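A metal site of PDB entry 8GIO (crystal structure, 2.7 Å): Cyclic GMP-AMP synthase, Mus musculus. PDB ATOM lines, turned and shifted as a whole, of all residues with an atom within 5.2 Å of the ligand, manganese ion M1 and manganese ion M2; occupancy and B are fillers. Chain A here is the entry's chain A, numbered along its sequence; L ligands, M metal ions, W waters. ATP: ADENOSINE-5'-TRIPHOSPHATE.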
ATOM      1  N   GLY A  55      13.611   8.893  -1.776  1.00  0.00           N
ATOM      2  CA  GLY A  55      14.770   8.500  -1.004  1.00  0.00           C
ATOM      3  C   GLY A  55      15.855   7.815  -1.826  1.00  0.00           C
ATOM      4  O   GLY A  55      15.803   7.760  -3.059  1.00  0.00           O
ATOM      5  N   SER A  56      16.855   7.287  -1.117  1.00  0.00           N
ATOM      6  CA  SER A  56      18.136   6.998  -1.768  1.00  0.00           C
ATOM      7  C   SER A  56      18.002   5.874  -2.775  1.00  0.00           C
ATOM      8  O   SER A  56      18.642   5.919  -3.846  1.00  0.00           O
ATOM      9  CB  SER A  56      19.217   6.663  -0.739  1.00  0.00           C
ATOM     10  OG  SER A  56      18.805   5.592   0.105  1.00  0.00           O
ATOM     11  N   TYR A  57      17.189   4.850  -2.473  1.00  0.00           N
ATOM     12  CA  TYR A  57      17.123   3.685  -3.354  1.00  0.00           C
ATOM     13  C   TYR A  57      16.631   4.066  -4.752  1.00  0.00           C
ATOM     14  O   TYR A  57      17.100   3.533  -5.754  1.00  0.00           O
ATOM     15  CB  TYR A  57      16.250   2.599  -2.740  1.00  0.00           C
ATOM     16  CG  TYR A  57      15.992   1.455  -3.693  1.00  0.00           C
ATOM     17  CD1 TYR A  57      16.905   0.403  -3.830  1.00  0.00           C
ATOM     18  CD2 TYR A  57      14.853   1.422  -4.473  1.00  0.00           C
ATOM     19  CE1 TYR A  57      16.672  -0.641  -4.704  1.00  0.00           C
ATOM     20  CE2 TYR A  57      14.605   0.392  -5.356  1.00  0.00           C
ATOM     21  CZ  TYR A  57      15.533  -0.631  -5.476  1.00  0.00           C
ATOM     22  OH  TYR A  57      15.260  -1.645  -6.359  1.00  0.00           O
ATOM     23  N   GLU A  59      16.794   7.280  -5.992  1.00  0.00           N
ATOM     24  CA  GLU A  59      17.760   8.184  -6.590  1.00  0.00           C
ATOM     25  C   GLU A  59      19.040   7.457  -7.015  1.00  0.00           C
ATOM     26  O   GLU A  59      19.890   8.075  -7.660  1.00  0.00           O
ATOM     27  CB  GLU A  59      18.105   9.322  -5.617  1.00  0.00           C
ATOM     28  CG  GLU A  59      16.875  10.122  -5.128  1.00  0.00           C
ATOM     29  CD  GLU A  59      17.067  10.801  -3.768  1.00  0.00           C
ATOM     30  OE1 GLU A  59      17.973  10.384  -2.994  1.00  0.00           O
ATOM     31  OE2 GLU A  59      16.325  11.765  -3.457  1.00  0.00           O
ATOM     32  N   LYS A  62      21.567   4.699  -2.727  1.00  0.00           N
ATOM     33  CA  LYS A  62      21.575   3.738  -1.621  1.00  0.00           C
ATOM     34  C   LYS A  62      22.862   2.936  -1.639  1.00  0.00           C
ATOM     35  O   LYS A  62      23.252   2.408  -2.684  1.00  0.00           O
ATOM     36  CB  LYS A  62      20.384   2.794  -1.750  1.00  0.00           C
ATOM     37  CG  LYS A  62      20.238   1.840  -0.610  1.00  0.00           C
ATOM     38  CD  LYS A  62      19.898   2.586   0.642  1.00  0.00           C
ATOM     39  CE  LYS A  62      19.615   1.641   1.793  1.00  0.00           C
ATOM     40  NZ  LYS A  62      20.827   1.226   2.523  1.00  0.00           N
ATOM     41  N   GLU A  68      16.765  -0.457   2.867  1.00  0.00           N
ATOM     42  CA  GLU A  68      15.944   0.631   3.404  1.00  0.00           C
ATOM     43  C   GLU A  68      15.303   1.415   2.272  1.00  0.00           C
ATOM     44  O   GLU A  68      15.993   2.125   1.548  1.00  0.00           O
ATOM     45  CB  GLU A  68      16.757   1.542   4.299  1.00  0.00           C
ATOM     46  CG  GLU A  68      15.925   2.207   5.351  1.00  0.00           C
ATOM     47  CD  GLU A  68      15.362   3.550   4.899  1.00  0.00           C
ATOM     48  OE1 GLU A  68      15.805   4.078   3.884  1.00  0.00           O
ATOM     49  OE2 GLU A  68      14.466   4.090   5.574  1.00  0.00           O
ATOM     50  N   PHE A  69      13.972   1.307   2.152  1.00  0.00           N
ATOM     51  CA  PHE A  69      13.186   1.928   1.096  1.00  0.00           C
ATOM     52  C   PHE A  69      12.256   2.951   1.705  1.00  0.00           C
ATOM     53  O   PHE A  69      11.734   2.756   2.809  1.00  0.00           O
ATOM     54  CB  PHE A  69      12.333   0.874   0.327  1.00  0.00           C
ATOM     55  CG  PHE A  69      13.149  -0.228  -0.284  1.00  0.00           C
ATOM     56  CD1 PHE A  69      13.748  -1.201   0.514  1.00  0.00           C
ATOM     57  CD2 PHE A  69      13.330  -0.285  -1.660  1.00  0.00           C
ATOM     58  CE1 PHE A  69      14.489  -2.193  -0.043  1.00  0.00           C
ATOM     59  CE2 PHE A  69      14.081  -1.274  -2.218  1.00  0.00           C
ATOM     60  CZ  PHE A  69      14.663  -2.222  -1.412  1.00  0.00           C
ATOM     61  N   ASP A  70      12.027   4.056   0.985  1.00  0.00           N
ATOM     62  CA  ASP A  70      11.071   5.064   1.435  1.00  0.00           C
ATOM     63  C   ASP A  70      10.012   5.262   0.377  1.00  0.00           C
ATOM     64  O   ASP A  70      10.332   5.396  -0.805  1.00  0.00           O
ATOM     65  CB  ASP A  70      11.735   6.409   1.729  1.00  0.00           C
ATOM     66  CG  ASP A  70      13.011   6.272   2.484  1.00  0.00           C
ATOM     67  OD1 ASP A  70      12.942   5.997   3.699  1.00  0.00           O
ATOM     68  OD2 ASP A  70      14.081   6.394   1.863  1.00  0.00           O
ATOM     69  N   ASP A 164       9.859   2.774   5.087  1.00  0.00           N
ATOM     70  CA  ASP A 164       9.126   3.876   5.692  1.00  0.00           C
ATOM     71  C   ASP A 164       7.928   4.246   4.813  1.00  0.00           C
ATOM     72  O   ASP A 164       8.109   4.829   3.737  1.00  0.00           O
ATOM     73  CB  ASP A 164      10.043   5.079   5.865  1.00  0.00           C
ATOM     74  CG  ASP A 164      11.117   4.837   6.868  1.00  0.00           C
ATOM     75  OD1 ASP A 164      10.829   4.150   7.863  1.00  0.00           O
ATOM     76  OD2 ASP A 164      12.249   5.315   6.689  1.00  0.00           O
ATOM     77  N   ARG A 221       5.056  19.304   8.473  1.00  0.00           N
ATOM     78  CA  ARG A 221       6.345  19.736   7.938  1.00  0.00           C
ATOM     79  C   ARG A 221       6.349  19.614   6.428  1.00  0.00           C
ATOM     80  O   ARG A 221       5.848  18.628   5.873  1.00  0.00           O
ATOM     81  CB  ARG A 221       7.498  18.892   8.526  1.00  0.00           C
ATOM     82  CG  ARG A 221       8.899  19.337   8.083  1.00  0.00           C
ATOM     83  CD  ARG A 221       9.938  18.218   8.152  1.00  0.00           C
ATOM     84  NE  ARG A 221      10.021  17.460   6.905  1.00  0.00           N
ATOM     85  CZ  ARG A 221      10.170  16.146   6.850  1.00  0.00           C
ATOM     86  NH1 ARG A 221      10.312  15.419   7.954  1.00  0.00           N
ATOM     87  NH2 ARG A 221      10.171  15.526   5.665  1.00  0.00           N
ATOM     88  N   LEU A 222       6.925  20.614   5.747  1.00  0.00           N
ATOM     89  CA  LEU A 222       7.023  20.557   4.283  1.00  0.00           C
ATOM     90  C   LEU A 222       7.964  19.426   3.864  1.00  0.00           C
ATOM     91  O   LEU A 222       8.928  19.107   4.566  1.00  0.00           O
ATOM     92  CB  LEU A 222       7.536  21.890   3.740  1.00  0.00           C
ATOM     93  CG  LEU A 222       6.533  23.035   3.597  1.00  0.00           C
ATOM     94  CD1 LEU A 222       7.169  24.380   3.399  1.00  0.00           C
ATOM     95  CD2 LEU A 222       5.608  22.725   2.423  1.00  0.00           C
ATOM     96  N   PHE A 224       9.998  17.786   0.262  1.00  0.00           N
ATOM     97  CA  PHE A 224      10.337  17.944  -1.138  1.00  0.00           C
ATOM     98  C   PHE A 224      11.041  16.709  -1.681  1.00  0.00           C
ATOM     99  O   PHE A 224      11.840  16.806  -2.610  1.00  0.00           O
ATOM    100  CB  PHE A 224      11.195  19.201  -1.339  1.00  0.00           C
ATOM    101  CG  PHE A 224      10.469  20.462  -1.005  1.00  0.00           C
ATOM    102  CD1 PHE A 224       9.581  21.030  -1.901  1.00  0.00           C
ATOM    103  CD2 PHE A 224      10.650  21.081   0.215  1.00  0.00           C
ATOM    104  CE1 PHE A 224       8.911  22.175  -1.620  1.00  0.00           C
ATOM    105  CE2 PHE A 224       9.978  22.248   0.529  1.00  0.00           C
ATOM    106  CZ  PHE A 224       9.092  22.799  -0.392  1.00  0.00           C
ATOM    107  N   SER A 225      10.783  15.527  -1.103  1.00  0.00           N
ATOM    108  CA  SER A 225      11.442  14.328  -1.589  1.00  0.00           C
ATOM    109  C   SER A 225      11.253  14.201  -3.081  1.00  0.00           C
ATOM    110  O   SER A 225      12.138  13.698  -3.770  1.00  0.00           O
ATOM    111  CB  SER A 225      10.903  13.066  -0.926  1.00  0.00           C
ATOM    112  OG  SER A 225      11.207  13.026   0.444  1.00  0.00           O
ATOM    113  N   GLU A 228      13.689  16.464  -4.870  1.00  0.00           N
ATOM    114  CA  GLU A 228      15.038  15.948  -4.700  1.00  0.00           C
ATOM    115  C   GLU A 228      15.290  14.702  -5.548  1.00  0.00           C
ATOM    116  O   GLU A 228      16.398  14.502  -6.051  1.00  0.00           O
ATOM    117  CB  GLU A 228      15.279  15.682  -3.223  1.00  0.00           C
ATOM    118  CG  GLU A 228      14.939  16.883  -2.340  1.00  0.00           C
ATOM    119  CD  GLU A 228      14.927  16.506  -0.876  1.00  0.00           C
ATOM    120  OE1 GLU A 228      15.275  15.347  -0.579  1.00  0.00           O
ATOM    121  OE2 GLU A 228      14.583  17.357  -0.027  1.00  0.00           O
ATOM    122  N   LYS A 259      27.805   9.863   2.436  1.00  0.00           N
ATOM    123  CA  LYS A 259      26.798   9.087   3.152  1.00  0.00           C
ATOM    124  C   LYS A 259      27.469   8.023   4.001  1.00  0.00           C
ATOM    125  O   LYS A 259      27.155   7.830   5.186  1.00  0.00           O
ATOM    126  CB  LYS A 259      25.821   8.438   2.172  1.00  0.00           C
ATOM    127  CG  LYS A 259      24.795   9.387   1.582  1.00  0.00           C
ATOM    128  CD  LYS A 259      24.119   8.752   0.371  1.00  0.00           C
ATOM    129  CE  LYS A 259      23.386   7.472   0.772  1.00  0.00           C
ATOM    130  NZ  LYS A 259      22.193   7.755   1.612  1.00  0.00           N
ATOM    131  N   GLU A 263      27.496   7.170   7.893  1.00  0.00           N
ATOM    132  CA  GLU A 263      26.899   5.922   8.365  1.00  0.00           C
ATOM    133  C   GLU A 263      27.860   5.167   9.279  1.00  0.00           C
ATOM    134  O   GLU A 263      27.468   4.663  10.340  1.00  0.00           O
ATOM    135  CB  GLU A 263      26.502   5.036   7.177  1.00  0.00           C
ATOM    136  CG  GLU A 263      25.133   5.305   6.630  1.00  0.00           C
ATOM    137  CD  GLU A 263      24.676   4.282   5.587  1.00  0.00           C
ATOM    138  OE1 GLU A 263      25.134   3.116   5.667  1.00  0.00           O
ATOM    139  OE2 GLU A 263      23.863   4.640   4.677  1.00  0.00           O
ATOM    140  N   CYS A 276      21.922  12.967  10.531  1.00  0.00           N
ATOM    141  CA  CYS A 276      21.180  12.075   9.663  1.00  0.00           C
ATOM    142  C   CYS A 276      21.667  12.296   8.242  1.00  0.00           C
ATOM    143  O   CYS A 276      22.390  13.240   7.964  1.00  0.00           O
ATOM    144  CB  CYS A 276      19.660  12.276   9.786  1.00  0.00           C
ATOM    145  SG  CYS A 276      18.998  13.785   9.053  1.00  0.00           S
ATOM    146  N   SER A 277      21.250  11.416   7.336  1.00  0.00           N
ATOM    147  CA  SER A 277      21.828  11.495   6.012  1.00  0.00           C
ATOM    148  C   SER A 277      21.314  12.717   5.260  1.00  0.00           C
ATOM    149  O   SER A 277      21.944  13.148   4.283  1.00  0.00           O
ATOM    150  CB  SER A 277      21.582  10.202   5.241  1.00  0.00           C
ATOM    151  OG  SER A 277      20.224  10.032   4.933  1.00  0.00           O
ATOM    152  N   TYR A 278      20.199  13.306   5.712  1.00  0.00           N
ATOM    153  CA  TYR A 278      19.657  14.459   5.003  1.00  0.00           C
ATOM    154  C   TYR A 278      20.570  15.667   5.148  1.00  0.00           C
ATOM    155  O   TYR A 278      20.647  16.521   4.249  1.00  0.00           O
ATOM    156  CB  TYR A 278      18.248  14.777   5.521  1.00  0.00           C
ATOM    157  CG  TYR A 278      17.501  15.771   4.665  1.00  0.00           C
ATOM    158  CD1 TYR A 278      17.052  15.427   3.396  1.00  0.00           C
ATOM    159  CD2 TYR A 278      17.237  17.079   5.125  1.00  0.00           C
ATOM    160  CE1 TYR A 278      16.346  16.326   2.581  1.00  0.00           C
ATOM    161  CE2 TYR A 278      16.546  18.001   4.319  1.00  0.00           C
ATOM    162  CZ  TYR A 278      16.101  17.606   3.047  1.00  0.00           C
ATOM    163  OH  TYR A 278      15.401  18.472   2.217  1.00  0.00           O
ATOM    164  N   LYS A 281      22.895  15.141   2.364  1.00  0.00           N
ATOM    165  CA  LYS A 281      22.248  15.456   1.096  1.00  0.00           C
ATOM    166  C   LYS A 281      22.116  16.949   0.904  1.00  0.00           C
ATOM    167  O   LYS A 281      22.361  17.478  -0.193  1.00  0.00           O
ATOM    168  CB  LYS A 281      20.868  14.791   1.050  1.00  0.00           C
ATOM    169  CG  LYS A 281      20.183  14.669  -0.305  1.00  0.00           C
ATOM    170  CD  LYS A 281      18.804  14.031  -0.106  1.00  0.00           C
ATOM    171  CE  LYS A 281      18.175  13.559  -1.433  1.00  0.00           C
ATOM    172  NZ  LYS A 281      16.762  13.070  -1.273  1.00  0.00           N
ATOM    173  N   HIS A 324      18.432  24.673   5.087  1.00  0.00           N
ATOM    174  CA  HIS A 324      17.556  23.873   4.259  1.00  0.00           C
ATOM    175  C   HIS A 324      17.599  24.383   2.829  1.00  0.00           C
ATOM    176  O   HIS A 324      17.527  25.589   2.589  1.00  0.00           O
ATOM    177  CB  HIS A 324      16.130  23.961   4.819  1.00  0.00           C
ATOM    178  CG  HIS A 324      15.216  22.880   4.340  1.00  0.00           C
ATOM    179  ND1 HIS A 324      14.890  22.713   3.009  1.00  0.00           N
ATOM    180  CD2 HIS A 324      14.545  21.918   5.015  1.00  0.00           C
ATOM    181  CE1 HIS A 324      14.066  21.686   2.882  1.00  0.00           C
ATOM    182  NE2 HIS A 324      13.846  21.185   4.082  1.00  0.00           N
HETATM  183  PG  ATP L   1      19.473   6.732   3.305  1.00  0.00           P
HETATM  184  O1G ATP L   1      20.378   7.170   4.418  1.00  0.00           O
HETATM  185  O2G ATP L   1      20.156   5.791   2.294  1.00  0.00           O
HETATM  186  O3G ATP L   1      18.178   6.124   3.824  1.00  0.00           O
HETATM  187  PB  ATP L   1      17.698   8.901   2.250  1.00  0.00           P
HETATM  188  O1B ATP L   1      17.913  10.214   1.608  1.00  0.00           O
HETATM  189  O2B ATP L   1      16.651   8.027   1.569  1.00  0.00           O
HETATM  190  O3B ATP L   1      18.995   7.997   2.430  1.00  0.00           O
HETATM  191  PA  ATP L   1      15.983   8.762   4.639  1.00  0.00           P
HETATM  192  O1A ATP L   1      16.315   9.018   6.044  1.00  0.00           O
HETATM  193  O2A ATP L   1      15.570   7.369   4.163  1.00  0.00           O
HETATM  194  O3A ATP L   1      17.254   9.103   3.755  1.00  0.00           O
HETATM  195  O5' ATP L   1      14.894   9.834   4.228  1.00  0.00           O
HETATM  196  C5' ATP L   1      14.051   9.653   3.071  1.00  0.00           C
HETATM  197  C4' ATP L   1      13.785  10.982   2.368  1.00  0.00           C
HETATM  198  O4' ATP L   1      12.928  11.794   3.203  1.00  0.00           O
HETATM  199  C3' ATP L   1      14.993  11.861   2.075  1.00  0.00           C
HETATM  200  O3' ATP L   1      15.580  11.549   0.816  1.00  0.00           O
HETATM  201  C2' ATP L   1      14.384  13.266   2.057  1.00  0.00           C
HETATM  202  O2' ATP L   1      13.699  13.553   0.842  1.00  0.00           O
HETATM  203  C1' ATP L   1      13.315  13.158   3.147  1.00  0.00           C
HETATM  204  N9  ATP L   1      13.764  13.565   4.471  1.00  0.00           N
HETATM  205  C8  ATP L   1      14.355  12.765   5.419  1.00  0.00           C
HETATM  206  N7  ATP L   1      14.666  13.395   6.531  1.00  0.00           N
HETATM  207  C5  ATP L   1      14.236  14.697   6.304  1.00  0.00           C
HETATM  208  C6  ATP L   1      14.281  15.856   7.091  1.00  0.00           C
HETATM  209  N6  ATP L   1      14.786  15.900   8.333  1.00  0.00           N
HETATM  210  N1  ATP L   1      13.753  17.000   6.568  1.00  0.00           N
HETATM  211  C2  ATP L   1      13.265  16.969   5.319  1.00  0.00           C
HETATM  212  N3  ATP L   1      13.192  15.933   4.485  1.00  0.00           N
HETATM  213  C4  ATP L   1      13.683  14.818   5.035  1.00  0.00           C
HETATM  214 MN    MN M   1      14.006   6.479   5.879  1.00  0.00          MN
HETATM  215 MN    MN M   2      16.500   5.743   2.394  1.00  0.00          MN
HETATM  216  O   HOH W   1      22.311   4.183   2.227  1.00  0.00           O
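Merely in contact with the ligand: Gly 55 (3.2 Å), Lys 62 (3.6 Å) and Tyr 278 (3.6 Å). Hydrophobic or aromatic side chains within 4 Å of the ligand: Tyr 278. Of the 21 residues printed, 12 come within 4 Å of the ligand.
Within 4 Å of manganese ion M1: Glu 68, Asp 70 and Asp 164.
N of Asp 164 is in hydrogen-bond range of O of Phe 69, at 3.0 Å. O of Ser 56 sits at hydrogen-bond distance from N of Lys 62 (3.4 Å). The side-chain carboxylate of Glu 228 is in salt-bridge range of the side-chain amino group of Lys 281, 2.8 Å away. The side-chain hydroxyl of Tyr 278 is in hydrogen-bond range of the side-chain carboxylate of Glu 228, 2.6 Å away. The side-chain amino group of Lys 281 is in salt-bridge range of the side-chain carboxylate of Glu 59, 2.6 Å away. The side-chain sulfur (SG) of Cys 276 sits close to the backbone NH (N) of Tyr 278, 3.6 Å away.
The side-chain hydroxyl (OG) of Ser 225 lies within hydrogen-bond range of an oxygen (O2') of the ligand (2.6 Å). The backbone NH of Ser 56 sits close to an oxygen (O2B) of the ligand, at 2.8 Å. The side-chain hydroxyl (OG) of Ser 56 sits at hydrogen-bond distance from an oxygen (O2G) of the ligand, at 2.6 Å. An oxygen (O2') of the ligand is in hydrogen-bond range of the side-chain carboxylate (OE1) of Glu 228, 2.8 Å away. The side-chain amino group (NZ) of Lys 281 lies within hydrogen-bond range of an oxygen (O3') of the ligand (2.8 Å). The side-chain amino group (NZ) of Lys 259 lies within salt-bridge range of an oxygen (O2G) of the ligand (2.9 Å). The side-chain hydroxyl of Ser 277 sits at hydrogen-bond distance from an oxygen (O1G) of the ligand (2.9 Å). NH2 of Arg 221 lies within hydrogen-bond range of N3 of the ligand, 3.3 Å away.
Water W1 lies within hydrogen-bond range of O2G of the ligand, OE2 of Glu 263 and NZ of Lys 62.
Manganese ion M1 is bound by OD2 of Asp 164, OE2 of Glu 68, OD1 of Asp 70 and O2A of the ligand. Manganese ion M1 has four donor atoms within binding distance.
Ser 56 touches manganese ion M2. Three residues have an atom within 4 Å of manganese ion M2: Ser 56, Glu 68 and Asp 70. The nearest printed residue that does not touch manganese ion M2 is Gly 55 (4.7 Å).
Manganese ion M2 is bound by an oxygen (O3G) of the ligand (2.2 Å), the side-chain carboxylate (OE1) of Glu 68 (2.3 Å), an oxygen (O2B) of the ligand (2.4 Å), the side-chain carboxylate (OD2) of Asp 70 (2.6 Å) and an oxygen (O2A) of the ligand (2.6 Å). Manganese ion M2 has five donor atoms within binding distance.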
